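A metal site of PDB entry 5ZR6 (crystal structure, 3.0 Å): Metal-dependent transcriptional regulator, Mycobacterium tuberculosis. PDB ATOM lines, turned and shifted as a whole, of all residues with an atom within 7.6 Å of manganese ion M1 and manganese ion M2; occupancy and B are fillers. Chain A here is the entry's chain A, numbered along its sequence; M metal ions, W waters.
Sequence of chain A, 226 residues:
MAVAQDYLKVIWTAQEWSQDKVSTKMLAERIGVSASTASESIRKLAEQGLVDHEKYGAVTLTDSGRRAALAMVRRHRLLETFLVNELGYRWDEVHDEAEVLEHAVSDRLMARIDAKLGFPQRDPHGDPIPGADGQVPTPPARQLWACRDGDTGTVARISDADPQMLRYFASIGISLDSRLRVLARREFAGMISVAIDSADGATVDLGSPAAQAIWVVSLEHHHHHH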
ATOM      1  N   LYS A   9     -34.483  24.298   8.687  1.00  0.00           N
ATOM      2  CA  LYS A   9     -33.243  23.716   8.211  1.00  0.00           C
ATOM      3  C   LYS A   9     -32.084  24.703   8.363  1.00  0.00           C
ATOM      4  O   LYS A   9     -30.979  24.315   8.736  1.00  0.00           O
ATOM      5  CB  LYS A   9     -33.377  23.282   6.753  1.00  0.00           C
ATOM      6  CG  LYS A   9     -32.183  22.487   6.243  1.00  0.00           C
ATOM      7  CD  LYS A   9     -32.134  22.397   4.731  1.00  0.00           C
ATOM      8  CE  LYS A   9     -32.081  23.781   4.100  1.00  0.00           C
ATOM      9  NZ  LYS A   9     -32.007  23.697   2.609  1.00  0.00           N
ATOM     10  N   THR A  13     -28.714  24.241  10.678  1.00  0.00           N
ATOM     11  CA  THR A  13     -27.389  24.208  10.060  1.00  0.00           C
ATOM     12  C   THR A  13     -26.475  25.278  10.645  1.00  0.00           C
ATOM     13  O   THR A  13     -25.260  25.075  10.725  1.00  0.00           O
ATOM     14  CB  THR A  13     -27.504  24.370   8.554  1.00  0.00           C
ATOM     15  OG1 THR A  13     -28.540  25.311   8.251  1.00  0.00           O
ATOM     16  CG2 THR A  13     -27.829  23.035   7.892  1.00  0.00           C
ATOM     17  N   HIS A  76     -32.372  17.147   2.134  1.00  0.00           N
ATOM     18  CA  HIS A  76     -31.412  17.970   1.405  1.00  0.00           C
ATOM     19  C   HIS A  76     -30.105  17.220   1.161  1.00  0.00           C
ATOM     20  O   HIS A  76     -29.561  17.242   0.058  1.00  0.00           O
ATOM     21  CB  HIS A  76     -31.141  19.265   2.181  1.00  0.00           C
ATOM     22  CG  HIS A  76     -30.078  20.127   1.562  1.00  0.00           C
ATOM     23  ND1 HIS A  76     -30.364  21.140   0.674  1.00  0.00           N
ATOM     24  CD2 HIS A  76     -28.739  20.131   1.713  1.00  0.00           C
ATOM     25  CE1 HIS A  76     -29.250  21.729   0.306  1.00  0.00           C
ATOM     26  NE2 HIS A  76     -28.241  21.137   0.921  1.00  0.00           N
ATOM     27  N   ARG A  77     -29.596  16.542   2.191  1.00  0.00           N
ATOM     28  CA  ARG A  77     -28.261  15.976   2.109  1.00  0.00           C
ATOM     29  C   ARG A  77     -28.241  14.637   1.390  1.00  0.00           C
ATOM     30  O   ARG A  77     -27.253  14.308   0.725  1.00  0.00           O
ATOM     31  CB  ARG A  77     -27.653  15.879   3.507  1.00  0.00           C
ATOM     32  CG  ARG A  77     -27.351  17.254   4.082  1.00  0.00           C
ATOM     33  CD  ARG A  77     -26.616  17.199   5.405  1.00  0.00           C
ATOM     34  NE  ARG A  77     -26.436  18.551   5.941  1.00  0.00           N
ATOM     35  CZ  ARG A  77     -25.793  18.831   7.062  1.00  0.00           C
ATOM     36  NH1 ARG A  77     -25.264  17.848   7.786  1.00  0.00           N
ATOM     37  NH2 ARG A  77     -25.678  20.083   7.470  1.00  0.00           N
ATOM     38  N   GLU A  80     -28.372  15.770  -2.338  1.00  0.00           N
ATOM     39  CA  GLU A  80     -27.030  16.118  -2.805  1.00  0.00           C
ATOM     40  C   GLU A  80     -26.229  14.874  -3.142  1.00  0.00           C
ATOM     41  O   GLU A  80     -25.583  14.786  -4.194  1.00  0.00           O
ATOM     42  CB  GLU A  80     -26.301  16.953  -1.758  1.00  0.00           C
ATOM     43  CG  GLU A  80     -26.905  18.325  -1.466  1.00  0.00           C
ATOM     44  CD  GLU A  80     -25.919  19.257  -0.782  1.00  0.00           C
ATOM     45  OE1 GLU A  80     -24.781  18.835  -0.533  1.00  0.00           O
ATOM     46  OE2 GLU A  80     -26.293  20.420  -0.507  1.00  0.00           O
ATOM     47  N   THR A  81     -26.274  13.883  -2.254  1.00  0.00           N
ATOM     48  CA  THR A  81     -25.526  12.647  -2.468  1.00  0.00           C
ATOM     49  C   THR A  81     -26.031  11.889  -3.678  1.00  0.00           C
ATOM     50  O   THR A  81     -25.237  11.319  -4.437  1.00  0.00           O
ATOM     51  CB  THR A  81     -25.596  11.772  -1.212  1.00  0.00           C
ATOM     52  OG1 THR A  81     -25.614  12.603  -0.053  1.00  0.00           O
ATOM     53  CG2 THR A  81     -24.408  10.819  -1.147  1.00  0.00           C
ATOM     54  N   TRP A  91     -19.716  18.451  -6.952  1.00  0.00           N
ATOM     55  CA  TRP A  91     -20.114  18.840  -5.603  1.00  0.00           C
ATOM     56  C   TRP A  91     -20.440  20.335  -5.489  1.00  0.00           C
ATOM     57  O   TRP A  91     -20.969  20.751  -4.442  1.00  0.00           O
ATOM     58  CB  TRP A  91     -19.030  18.444  -4.590  1.00  0.00           C
ATOM     59  CG  TRP A  91     -17.680  19.093  -4.751  1.00  0.00           C
ATOM     60  CD1 TRP A  91     -17.226  19.788  -5.843  1.00  0.00           C
ATOM     61  CD2 TRP A  91     -16.612  19.090  -3.804  1.00  0.00           C
ATOM     62  NE1 TRP A  91     -15.942  20.215  -5.614  1.00  0.00           N
ATOM     63  CE2 TRP A  91     -15.540  19.805  -4.370  1.00  0.00           C
ATOM     64  CE3 TRP A  91     -16.469  18.548  -2.517  1.00  0.00           C
ATOM     65  CZ2 TRP A  91     -14.337  19.992  -3.696  1.00  0.00           C
ATOM     66  CZ3 TRP A  91     -15.262  18.737  -1.852  1.00  0.00           C
ATOM     67  CH2 TRP A  91     -14.221  19.455  -2.440  1.00  0.00           C
ATOM     68  N   VAL A  94     -24.660  20.733  -6.659  1.00  0.00           N
ATOM     69  CA  VAL A  94     -25.716  19.975  -5.986  1.00  0.00           C
ATOM     70  C   VAL A  94     -26.545  20.824  -5.017  1.00  0.00           C
ATOM     71  O   VAL A  94     -27.712  20.504  -4.783  1.00  0.00           O
ATOM     72  CB  VAL A  94     -25.124  18.758  -5.249  1.00  0.00           C
ATOM     73  CG1 VAL A  94     -24.558  17.785  -6.229  1.00  0.00           C
ATOM     74  CG2 VAL A  94     -24.055  19.202  -4.264  1.00  0.00           C
ATOM     75  N   HIS A  95     -25.967  21.876  -4.441  1.00  0.00           N
ATOM     76  CA  HIS A  95     -26.671  22.551  -3.349  1.00  0.00           C
ATOM     77  C   HIS A  95     -27.867  23.338  -3.857  1.00  0.00           C
ATOM     78  O   HIS A  95     -28.939  23.321  -3.231  1.00  0.00           O
ATOM     79  CB  HIS A  95     -25.718  23.454  -2.585  1.00  0.00           C
ATOM     80  CG  HIS A  95     -26.318  24.016  -1.333  1.00  0.00           C
ATOM     81  ND1 HIS A  95     -26.385  23.306  -0.155  1.00  0.00           N
ATOM     82  CD2 HIS A  95     -26.905  25.217  -1.076  1.00  0.00           C
ATOM     83  CE1 HIS A  95     -26.974  24.046   0.776  1.00  0.00           C
ATOM     84  NE2 HIS A  95     -27.302  25.197   0.233  1.00  0.00           N
ATOM     85  N   ASP A  96     -27.715  24.049  -4.971  1.00  0.00           N
ATOM     86  CA  ASP A  96     -28.841  24.808  -5.502  1.00  0.00           C
ATOM     87  C   ASP A  96     -29.965  23.894  -5.986  1.00  0.00           C
ATOM     88  O   ASP A  96     -31.144  24.273  -5.933  1.00  0.00           O
ATOM     89  CB  ASP A  96     -28.374  25.724  -6.636  1.00  0.00           C
ATOM     90  CG  ASP A  96     -27.284  26.686  -6.178  1.00  0.00           C
ATOM     91  OD1 ASP A  96     -27.244  27.006  -4.981  1.00  0.00           O
ATOM     92  OD2 ASP A  96     -26.487  27.118  -7.038  1.00  0.00           O
ATOM     93  N   ALA A  98     -30.721  20.578  -4.740  1.00  0.00           N
ATOM     94  CA  ALA A  98     -31.389  19.998  -3.588  1.00  0.00           C
ATOM     95  C   ALA A  98     -32.058  21.041  -2.709  1.00  0.00           C
ATOM     96  O   ALA A  98     -32.917  20.698  -1.899  1.00  0.00           O
ATOM     97  CB  ALA A  98     -30.389  19.187  -2.756  1.00  0.00           C
ATOM     98  N   GLU A  99     -31.697  22.323  -2.865  1.00  0.00           N
ATOM     99  CA  GLU A  99     -32.382  23.371  -2.120  1.00  0.00           C
ATOM    100  C   GLU A  99     -33.817  23.559  -2.608  1.00  0.00           C
ATOM    101  O   GLU A  99     -34.678  24.001  -1.854  1.00  0.00           O
ATOM    102  CB  GLU A  99     -31.601  24.680  -2.234  1.00  0.00           C
ATOM    103  CG  GLU A  99     -32.173  25.843  -1.427  1.00  0.00           C
ATOM    104  CD  GLU A  99     -32.067  25.626   0.066  1.00  0.00           C
ATOM    105  OE1 GLU A  99     -30.998  25.185   0.535  1.00  0.00           O
ATOM    106  OE2 GLU A  99     -33.052  25.899   0.777  1.00  0.00           O
ATOM    107  N   GLU A 102     -35.995  19.761  -2.139  1.00  0.00           N
ATOM    108  CA  GLU A 102     -36.246  19.301  -0.778  1.00  0.00           C
ATOM    109  C   GLU A 102     -37.710  19.420  -0.370  1.00  0.00           C
ATOM    110  O   GLU A 102     -38.139  18.693   0.530  1.00  0.00           O
ATOM    111  CB  GLU A 102     -35.367  20.086   0.197  1.00  0.00           C
ATOM    112  CG  GLU A 102     -35.558  21.586   0.135  1.00  0.00           C
ATOM    113  CD  GLU A 102     -34.508  22.350   0.899  1.00  0.00           C
ATOM    114  OE1 GLU A 102     -34.651  23.585   1.057  1.00  0.00           O
ATOM    115  OE2 GLU A 102     -33.508  21.729   1.332  1.00  0.00           O
ATOM    116  N   ARG A 122     -22.710  10.630   4.965  1.00  0.00           N
ATOM    117  CA  ARG A 122     -22.117  11.941   4.749  1.00  0.00           C
ATOM    118  C   ARG A 122     -22.331  12.390   3.311  1.00  0.00           C
ATOM    119  O   ARG A 122     -22.561  11.581   2.411  1.00  0.00           O
ATOM    120  CB  ARG A 122     -20.629  11.936   5.116  1.00  0.00           C
ATOM    121  CG  ARG A 122     -19.691  11.428   4.033  1.00  0.00           C
ATOM    122  CD  ARG A 122     -18.253  11.714   4.412  1.00  0.00           C
ATOM    123  NE  ARG A 122     -17.293  11.122   3.483  1.00  0.00           N
ATOM    124  CZ  ARG A 122     -16.016  10.879   3.784  1.00  0.00           C
ATOM    125  NH1 ARG A 122     -15.546  11.181   4.986  1.00  0.00           N
ATOM    126  NH2 ARG A 122     -15.213  10.341   2.883  1.00  0.00           N
ATOM    127  N   ASP A 123     -22.266  13.703   3.127  1.00  0.00           N
ATOM    128  CA  ASP A 123     -22.488  14.410   1.873  1.00  0.00           C
ATOM    129  C   ASP A 123     -21.376  14.165   0.869  1.00  0.00           C
ATOM    130  O   ASP A 123     -20.386  13.494   1.181  1.00  0.00           O
ATOM    131  CB  ASP A 123     -22.601  15.910   2.132  1.00  0.00           C
ATOM    132  CG  ASP A 123     -24.024  16.401   2.125  1.00  0.00           C
ATOM    133  OD1 ASP A 123     -24.937  15.541   2.173  1.00  0.00           O
ATOM    134  OD2 ASP A 123     -24.229  17.629   2.074  1.00  0.00           O
ATOM    135  N   PRO A 124     -21.498  14.689  -0.359  1.00  0.00           N
ATOM    136  CA  PRO A 124     -20.299  14.920  -1.170  1.00  0.00           C
ATOM    137  C   PRO A 124     -19.358  15.915  -0.535  1.00  0.00           C
ATOM    138  O   PRO A 124     -18.173  15.952  -0.889  1.00  0.00           O
ATOM    139  CB  PRO A 124     -20.862  15.435  -2.499  1.00  0.00           C
ATOM    140  CG  PRO A 124     -22.259  14.885  -2.542  1.00  0.00           C
ATOM    141  CD  PRO A 124     -22.735  14.927  -1.132  1.00  0.00           C
ATOM    142  N   HIS A 125     -19.855  16.728   0.399  1.00  0.00           N
ATOM    143  CA  HIS A 125     -19.047  17.679   1.151  1.00  0.00           C
ATOM    144  C   HIS A 125     -18.657  17.150   2.531  1.00  0.00           C
ATOM    145  O   HIS A 125     -17.980  17.859   3.277  1.00  0.00           O
ATOM    146  CB  HIS A 125     -19.799  19.006   1.325  1.00  0.00           C
ATOM    147  CG  HIS A 125     -20.516  19.449   0.089  1.00  0.00           C
ATOM    148  ND1 HIS A 125     -21.824  19.873   0.102  1.00  0.00           N
ATOM    149  CD2 HIS A 125     -20.098  19.556  -1.196  1.00  0.00           C
ATOM    150  CE1 HIS A 125     -22.185  20.214  -1.129  1.00  0.00           C
ATOM    151  NE2 HIS A 125     -21.157  20.036  -1.925  1.00  0.00           N
ATOM    152  N   GLY A 126     -19.065  15.934   2.876  1.00  0.00           N
ATOM    153  CA  GLY A 126     -18.834  15.405   4.208  1.00  0.00           C
ATOM    154  C   GLY A 126     -19.857  15.830   5.235  1.00  0.00           C
ATOM    155  O   GLY A 126     -19.716  15.448   6.409  1.00  0.00           O
ATOM    156  N   ASP A 127     -20.860  16.608   4.850  1.00  0.00           N
ATOM    157  CA  ASP A 127     -21.919  16.991   5.770  1.00  0.00           C
ATOM    158  C   ASP A 127     -22.628  15.744   6.289  1.00  0.00           C
ATOM    159  O   ASP A 127     -23.050  14.899   5.484  1.00  0.00           O
ATOM    160  CB  ASP A 127     -22.925  17.915   5.086  1.00  0.00           C
ATOM    161  CG  ASP A 127     -22.328  19.252   4.692  1.00  0.00           C
ATOM    162  OD1 ASP A 127     -21.232  19.586   5.191  1.00  0.00           O
ATOM    163  OD2 ASP A 127     -22.962  19.982   3.895  1.00  0.00           O
ATOM    164  N   PRO A 128     -22.770  15.580   7.602  1.00  0.00           N
ATOM    165  CA  PRO A 128     -23.382  14.348   8.117  1.00  0.00           C
ATOM    166  C   PRO A 128     -24.856  14.267   7.761  1.00  0.00           C
ATOM    167  O   PRO A 128     -25.597  15.249   7.867  1.00  0.00           O
ATOM    168  CB  PRO A 128     -23.172  14.476   9.635  1.00  0.00           C
ATOM    169  CG  PRO A 128     -23.123  15.939   9.883  1.00  0.00           C
ATOM    170  CD  PRO A 128     -22.434  16.529   8.676  1.00  0.00           C
ATOM    171  N   ARG A 157     -15.063  17.691   6.417  1.00  0.00           N
ATOM    172  CA  ARG A 157     -16.259  18.400   5.992  1.00  0.00           C
ATOM    173  C   ARG A 157     -15.847  19.747   5.401  1.00  0.00           C
ATOM    174  O   ARG A 157     -15.020  20.448   5.986  1.00  0.00           O
ATOM    175  CB  ARG A 157     -17.227  18.595   7.171  1.00  0.00           C
ATOM    176  CG  ARG A 157     -18.577  19.231   6.816  1.00  0.00           C
ATOM    177  CD  ARG A 157     -18.579  20.750   6.795  1.00  0.00           C
ATOM    178  NE  ARG A 157     -19.934  21.278   6.679  1.00  0.00           N
ATOM    179  CZ  ARG A 157     -20.245  22.573   6.698  1.00  0.00           C
ATOM    180  NH1 ARG A 157     -19.295  23.481   6.824  1.00  0.00           N
ATOM    181  NH2 ARG A 157     -21.515  22.953   6.586  1.00  0.00           N
ATOM    182  N   ILE A 158     -16.425  20.095   4.254  1.00  0.00           N
ATOM    183  CA  ILE A 158     -16.160  21.353   3.583  1.00  0.00           C
ATOM    184  C   ILE A 158     -17.491  22.069   3.368  1.00  0.00           C
ATOM    185  O   ILE A 158     -18.436  21.474   2.846  1.00  0.00           O
ATOM    186  CB  ILE A 158     -15.418  21.154   2.254  1.00  0.00           C
ATOM    187  CG1 ILE A 158     -14.134  20.347   2.478  1.00  0.00           C
ATOM    188  CG2 ILE A 158     -15.112  22.501   1.614  1.00  0.00           C
ATOM    189  CD1 ILE A 158     -13.236  20.272   1.273  1.00  0.00           C
ATOM    190  N   SER A 159     -17.545  23.342   3.771  1.00  0.00           N
ATOM    191  CA  SER A 159     -18.751  24.131   3.572  1.00  0.00           C
ATOM    192  C   SER A 159     -19.058  24.288   2.091  1.00  0.00           C
ATOM    193  O   SER A 159     -18.159  24.333   1.244  1.00  0.00           O
ATOM    194  CB  SER A 159     -18.599  25.507   4.210  1.00  0.00           C
ATOM    195  OG  SER A 159     -19.734  26.326   3.958  1.00  0.00           O
ATOM    196  N   ASP A 160     -20.353  24.375   1.778  1.00  0.00           N
ATOM    197  CA  ASP A 160     -20.798  24.545   0.399  1.00  0.00           C
ATOM    198  C   ASP A 160     -21.494  25.895   0.188  1.00  0.00           C
ATOM    199  O   ASP A 160     -22.236  26.052  -0.784  1.00  0.00           O
ATOM    200  CB  ASP A 160     -21.711  23.390  -0.017  1.00  0.00           C
ATOM    201  CG  ASP A 160     -23.070  23.406   0.693  1.00  0.00           C
ATOM    202  OD1 ASP A 160     -23.250  24.178   1.652  1.00  0.00           O
ATOM    203  OD2 ASP A 160     -23.945  22.636   0.274  1.00  0.00           O
ATOM    204  N   ALA A 161     -21.255  26.853   1.075  1.00  0.00           N
ATOM    205  CA  ALA A 161     -21.888  28.165   0.924  1.00  0.00           C
ATOM    206  C   ALA A 161     -21.407  28.879  -0.327  1.00  0.00           C
ATOM    207  O   ALA A 161     -22.155  29.692  -0.903  1.00  0.00           O
ATOM    208  CB  ALA A 161     -21.628  29.015   2.157  1.00  0.00           C
HETATM  209 MN    MN M   1     -23.922  19.309   1.764  1.00  0.00          MN
HETATM  210 MN    MN M   2     -26.002  21.709   1.086  1.00  0.00          MN
HETATM  211  O   HOH W   1     -25.303  21.537   3.359  1.00  0.00           O
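Manganese ion M2 is bound by ND1 of His 95 (2.1 Å), OE2 of Glu 80 (2.1 Å), NE2 of His 76 (2.3 Å), water W1 (2.4 Å) and OD2 of Asp 160 (2.4 Å).
The nearest printed residue that does not touch manganese ion M1 is Arg 77 (4.6 Å).
Manganese ion M1 is bound by OD2 of Asp 123 (1.7 Å).
Manganese ion M1 is bound by OD2 of Asp 127, at 2.4 Å.
Manganese ion M1 is bound by the side-chain carboxylate (OE1) of Glu 80.
Slightly farther from manganese ion M1 lies ND1 of His 125 (2.7 Å).
OD2 of Asp 160 sits close to ND1 of His 125 (3.5 Å).
O of His 125 is in hydrogen-bond range of N of Ile 158.
A ring nitrogen (ND1) of His 76 lies within hydrogen-bond range of the side-chain carboxylate of Glu 102, at 3.3 Å.
The side-chain carboxylate (OE1) of Glu 80 lies close to a ring nitrogen (ND1) of His 125 (3.2 Å).
A ring nitrogen (NE2) of His 125 lies within hydrogen-bond range of the backbone carbonyl oxygen of Trp 91 (2.6 Å).
The side-chain carboxylate (OD1) of Asp 127 is in salt-bridge range of the guanidinium group (NE) of Arg 157.
Of the 25 residues printed, 4 come within 4 Å of manganese ion M2.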
